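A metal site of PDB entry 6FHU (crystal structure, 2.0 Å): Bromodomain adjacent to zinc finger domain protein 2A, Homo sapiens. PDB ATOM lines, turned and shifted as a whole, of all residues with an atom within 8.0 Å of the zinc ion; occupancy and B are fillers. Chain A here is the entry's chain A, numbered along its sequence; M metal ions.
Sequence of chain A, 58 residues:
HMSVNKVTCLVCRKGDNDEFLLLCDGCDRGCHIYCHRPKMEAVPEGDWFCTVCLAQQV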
ATOM      1  N   THR A   8      13.524 -21.755   3.216  1.00  0.00           N
ATOM      2  CA  THR A   8      13.097 -21.046   4.406  1.00  0.00           C
ATOM      3  C   THR A   8      14.330 -20.557   5.195  1.00  0.00           C
ATOM      4  O   THR A   8      15.390 -21.193   5.172  1.00  0.00           O
ATOM      5  CB  THR A   8      12.196 -21.997   5.207  1.00  0.00           C
ATOM      6  OG1 THR A   8      10.888 -21.943   4.629  1.00  0.00           O
ATOM      7  CG2 THR A   8      12.092 -21.633   6.666  1.00  0.00           C
ATOM      8  N   CYS A   9      14.176 -19.434   5.887  1.00  0.00           N
ATOM      9  CA  CYS A   9      15.240 -18.837   6.695  1.00  0.00           C
ATOM     10  C   CYS A   9      15.443 -19.584   8.035  1.00  0.00           C
ATOM     11  O   CYS A   9      14.503 -19.798   8.795  1.00  0.00           O
ATOM     12  CB  CYS A   9      14.922 -17.348   6.928  1.00  0.00           C
ATOM     13  SG  CYS A   9      15.995 -16.441   8.082  1.00  0.00           S
ATOM     14  N   LEU A  10      16.679 -19.969   8.309  1.00  0.00           N
ATOM     15  CA  LEU A  10      17.021 -20.681   9.565  1.00  0.00           C
ATOM     16  C   LEU A  10      16.678 -19.895  10.832  1.00  0.00           C
ATOM     17  O   LEU A  10      16.311 -20.500  11.837  1.00  0.00           O
ATOM     18  CB  LEU A  10      18.507 -21.016   9.599  1.00  0.00           C
ATOM     19  CG  LEU A  10      19.053 -22.049   8.613  1.00  0.00           C
ATOM     20  CD1 LEU A  10      20.580 -22.107   8.630  1.00  0.00           C
ATOM     21  CD2 LEU A  10      18.476 -23.423   8.922  1.00  0.00           C
ATOM     22  N   VAL A  11      16.802 -18.576  10.801  1.00  0.00           N
ATOM     23  CA  VAL A  11      16.542 -17.763  11.982  1.00  0.00           C
ATOM     24  C   VAL A  11      15.032 -17.576  12.244  1.00  0.00           C
ATOM     25  O   VAL A  11      14.527 -17.997  13.269  1.00  0.00           O
ATOM     26  CB  VAL A  11      17.232 -16.381  11.874  1.00  0.00           C
ATOM     27  CG1 VAL A  11      16.964 -15.513  13.104  1.00  0.00           C
ATOM     28  CG2 VAL A  11      18.740 -16.574  11.641  1.00  0.00           C
ATOM     29  N   CYS A  12      14.337 -16.933  11.306  1.00  0.00           N
ATOM     30  CA  CYS A  12      12.909 -16.577  11.475  1.00  0.00           C
ATOM     31  C   CYS A  12      11.914 -17.592  10.908  1.00  0.00           C
ATOM     32  O   CYS A  12      10.725 -17.414  11.087  1.00  0.00           O
ATOM     33  CB  CYS A  12      12.629 -15.210  10.844  1.00  0.00           C
ATOM     34  SG  CYS A  12      12.586 -15.219   9.035  1.00  0.00           S
ATOM     35  N   ARG A  13      12.388 -18.635  10.198  1.00  0.00           N
ATOM     36  CA  ARG A  13      11.524 -19.719   9.686  1.00  0.00           C
ATOM     37  C   ARG A  13      10.502 -19.294   8.588  1.00  0.00           C
ATOM     38  O   ARG A  13       9.580 -20.054   8.279  1.00  0.00           O
ATOM     39  CB  ARG A  13      10.779 -20.445  10.840  1.00  0.00           C
ATOM     40  CG  ARG A  13      11.665 -21.010  11.937  1.00  0.00           C
ATOM     41  CD  ARG A  13      12.266 -22.348  11.554  1.00  0.00           C
ATOM     42  NE  ARG A  13      13.701 -22.426  11.865  1.00  0.00           N
ATOM     43  CZ  ARG A  13      14.543 -23.397  11.466  1.00  0.00           C
ATOM     44  NH1 ARG A  13      14.113 -24.430  10.735  1.00  0.00           N
ATOM     45  NH2 ARG A  13      15.831 -23.329  11.810  1.00  0.00           N
ATOM     46  N   LYS A  14      10.679 -18.119   7.982  1.00  0.00           N
ATOM     47  CA  LYS A  14       9.813 -17.671   6.896  1.00  0.00           C
ATOM     48  C   LYS A  14      10.583 -17.689   5.585  1.00  0.00           C
ATOM     49  O   LYS A  14      11.822 -17.650   5.577  1.00  0.00           O
ATOM     50  CB  LYS A  14       9.269 -16.277   7.167  1.00  0.00           C
ATOM     51  CG  LYS A  14       8.582 -16.134   8.512  1.00  0.00           C
ATOM     52  CD  LYS A  14       8.029 -14.730   8.696  1.00  0.00           C
ATOM     53  CE  LYS A  14       7.336 -14.583  10.049  1.00  0.00           C
ATOM     54  NZ  LYS A  14       6.723 -13.230  10.236  1.00  0.00           N
ATOM     55  N   GLY A  15       9.836 -17.757   4.487  1.00  0.00           N
ATOM     56  CA  GLY A  15      10.387 -17.788   3.130  1.00  0.00           C
ATOM     57  C   GLY A  15      10.011 -16.571   2.290  1.00  0.00           C
ATOM     58  O   GLY A  15      10.196 -16.586   1.074  1.00  0.00           O
ATOM     59  N   ASP A  16       9.490 -15.518   2.936  1.00  0.00           N
ATOM     60  CA  ASP A  16       9.151 -14.257   2.252  1.00  0.00           C
ATOM     61  C   ASP A  16      10.402 -13.434   1.901  1.00  0.00           C
ATOM     62  O   ASP A  16      11.505 -13.742   2.347  1.00  0.00           O
ATOM     63  CB  ASP A  16       8.133 -13.425   3.067  1.00  0.00           C
ATOM     64  CG  ASP A  16       8.584 -13.128   4.499  1.00  0.00           C
ATOM     65  OD1 ASP A  16       9.724 -13.462   4.891  1.00  0.00           O
ATOM     66  OD2 ASP A  16       7.770 -12.559   5.254  1.00  0.00           O
ATOM     67  N   PHE A  20      16.076 -11.067  -0.643  1.00  0.00           N
ATOM     68  CA  PHE A  20      16.949 -10.915   0.550  1.00  0.00           C
ATOM     69  C   PHE A  20      17.433 -12.252   1.161  1.00  0.00           C
ATOM     70  O   PHE A  20      18.199 -12.257   2.140  1.00  0.00           O
ATOM     71  CB  PHE A  20      16.205 -10.090   1.620  1.00  0.00           C
ATOM     72  CG  PHE A  20      16.032  -8.658   1.254  1.00  0.00           C
ATOM     73  CD1 PHE A  20      14.924  -8.232   0.518  1.00  0.00           C
ATOM     74  CD2 PHE A  20      16.967  -7.701   1.654  1.00  0.00           C
ATOM     75  CE1 PHE A  20      14.762  -6.900   0.174  1.00  0.00           C
ATOM     76  CE2 PHE A  20      16.802  -6.355   1.315  1.00  0.00           C
ATOM     77  CZ  PHE A  20      15.706  -5.957   0.575  1.00  0.00           C
ATOM     78  N   LEU A  21      17.026 -13.372   0.557  1.00  0.00           N
ATOM     79  CA  LEU A  21      17.140 -14.694   1.159  1.00  0.00           C
ATOM     80  C   LEU A  21      18.307 -15.457   0.542  1.00  0.00           C
ATOM     81  O   LEU A  21      18.182 -15.943  -0.602  1.00  0.00           O
ATOM     82  CB  LEU A  21      15.838 -15.473   0.940  1.00  0.00           C
ATOM     83  CG  LEU A  21      15.675 -16.870   1.508  1.00  0.00           C
ATOM     84  CD1 LEU A  21      15.833 -16.862   3.026  1.00  0.00           C
ATOM     85  CD2 LEU A  21      14.322 -17.438   1.108  1.00  0.00           C
ATOM     86  N   GLY A  30      18.767 -21.758   4.053  1.00  0.00           N
ATOM     87  CA  GLY A  30      18.825 -20.340   3.730  1.00  0.00           C
ATOM     88  C   GLY A  30      18.796 -19.417   4.912  1.00  0.00           C
ATOM     89  O   GLY A  30      18.578 -19.865   6.051  1.00  0.00           O
ATOM     90  N   CYS A  31      18.998 -18.128   4.646  1.00  0.00           N
ATOM     91  CA  CYS A  31      18.965 -17.096   5.690  1.00  0.00           C
ATOM     92  C   CYS A  31      18.782 -15.700   5.087  1.00  0.00           C
ATOM     93  O   CYS A  31      19.525 -15.326   4.188  1.00  0.00           O
ATOM     94  CB  CYS A  31      20.259 -17.132   6.523  1.00  0.00           C
ATOM     95  SG  CYS A  31      20.316 -16.029   7.946  1.00  0.00           S
ATOM     96  N   HIS A  32      17.803 -14.937   5.596  1.00  0.00           N
ATOM     97  CA  HIS A  32      17.625 -13.516   5.217  1.00  0.00           C
ATOM     98  C   HIS A  32      18.869 -12.736   5.617  1.00  0.00           C
ATOM     99  O   HIS A  32      19.391 -12.947   6.710  1.00  0.00           O
ATOM    100  CB  HIS A  32      16.436 -12.891   5.935  1.00  0.00           C
ATOM    101  CG  HIS A  32      15.112 -13.461   5.535  1.00  0.00           C
ATOM    102  ND1 HIS A  32      14.315 -14.181   6.403  1.00  0.00           N
ATOM    103  CD2 HIS A  32      14.435 -13.385   4.362  1.00  0.00           C
ATOM    104  CE1 HIS A  32      13.211 -14.555   5.769  1.00  0.00           C
ATOM    105  NE2 HIS A  32      13.258 -14.083   4.533  1.00  0.00           N
ATOM    106  N   ILE A  33      19.347 -11.845   4.757  1.00  0.00           N
ATOM    107  CA  ILE A  33      20.524 -11.046   5.100  1.00  0.00           C
ATOM    108  C   ILE A  33      20.224 -10.195   6.341  1.00  0.00           C
ATOM    109  O   ILE A  33      21.102  -9.998   7.176  1.00  0.00           O
ATOM    110  CB  ILE A  33      21.080 -10.184   3.947  1.00  0.00           C
ATOM    111  CG1 ILE A  33      20.114  -9.086   3.501  1.00  0.00           C
ATOM    112  CG2 ILE A  33      21.490 -11.061   2.763  1.00  0.00           C
ATOM    113  CD1 ILE A  33      20.700  -8.204   2.409  1.00  0.00           C
ATOM    114  N   TYR A  34      18.976  -9.778   6.478  1.00  0.00           N
ATOM    115  CA  TYR A  34      18.538  -8.971   7.631  1.00  0.00           C
ATOM    116  C   TYR A  34      18.364  -9.737   8.946  1.00  0.00           C
ATOM    117  O   TYR A  34      18.320  -9.128   9.999  1.00  0.00           O
ATOM    118  CB  TYR A  34      17.259  -8.150   7.291  1.00  0.00           C
ATOM    119  CG  TYR A  34      16.052  -8.904   6.749  1.00  0.00           C
ATOM    120  CD1 TYR A  34      15.204  -9.619   7.583  1.00  0.00           C
ATOM    121  CD2 TYR A  34      15.739  -8.853   5.379  1.00  0.00           C
ATOM    122  CE1 TYR A  34      14.088 -10.285   7.074  1.00  0.00           C
ATOM    123  CE2 TYR A  34      14.619  -9.509   4.861  1.00  0.00           C
ATOM    124  CZ  TYR A  34      13.789 -10.218   5.708  1.00  0.00           C
ATOM    125  OH  TYR A  34      12.693 -10.876   5.168  1.00  0.00           O
ATOM    126  N   CYS A  35      18.283 -11.070   8.877  1.00  0.00           N
ATOM    127  CA  CYS A  35      18.307 -11.918  10.083  1.00  0.00           C
ATOM    128  C   CYS A  35      19.706 -12.346  10.514  1.00  0.00           C
ATOM    129  O   CYS A  35      19.867 -12.804  11.639  1.00  0.00           O
ATOM    130  CB  CYS A  35      17.435 -13.167   9.876  1.00  0.00           C
ATOM    131  SG  CYS A  35      15.700 -12.782   9.573  1.00  0.00           S
ATOM    132  N   HIS A  36      20.708 -12.190   9.639  1.00  0.00           N
ATOM    133  CA  HIS A  36      22.104 -12.594   9.938  1.00  0.00           C
ATOM    134  C   HIS A  36      22.733 -11.687  11.010  1.00  0.00           C
ATOM    135  O   HIS A  36      22.499 -10.484  11.011  1.00  0.00           O
ATOM    136  CB  HIS A  36      22.970 -12.548   8.663  1.00  0.00           C
ATOM    137  CG  HIS A  36      24.212 -13.402   8.723  1.00  0.00           C
ATOM    138  ND1 HIS A  36      25.379 -12.973   9.324  1.00  0.00           N
ATOM    139  CD2 HIS A  36      24.475 -14.638   8.224  1.00  0.00           C
ATOM    140  CE1 HIS A  36      26.301 -13.919   9.204  1.00  0.00           C
ATOM    141  NE2 HIS A  36      25.782 -14.945   8.547  1.00  0.00           N
HETATM  142 ZN    ZN M   1      14.729 -14.502   8.370  1.00  0.00          ZN
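NE2 of His 32 sits close to OH of Tyr 34 (3.3 Å).
NE2 of His 32 lies within hydrogen-bond range of O of Asp 16, 2.8 Å away.
The backbone NH (N) of Val 11 sits close to the side-chain sulfur (SG) of Cys 9, at 3.5 Å.
O of Lys 14 is in hydrogen-bond range of N of Cys 9, at 3.0 Å.
N of Lys 14 lies close to SG of Cys 12 (3.6 Å).
Four residues have an atom within 4 Å of the zinc ion: Cys 9, Cys 12, His 32 and Cys 35.
The nearest printed residue that does not touch the zinc ion is Tyr 34 (4.5 Å).
The zinc ion is bound by ND1 of His 32 (2.0 Å).
The side-chain sulfur (SG) of Cys 35 binds the zinc ion (2.3 Å).
The zinc ion is bound by SG of Cys 9, 2.3 Å away.
The zinc ion is bound by the side-chain sulfur (SG) of Cys 12 (2.4 Å).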
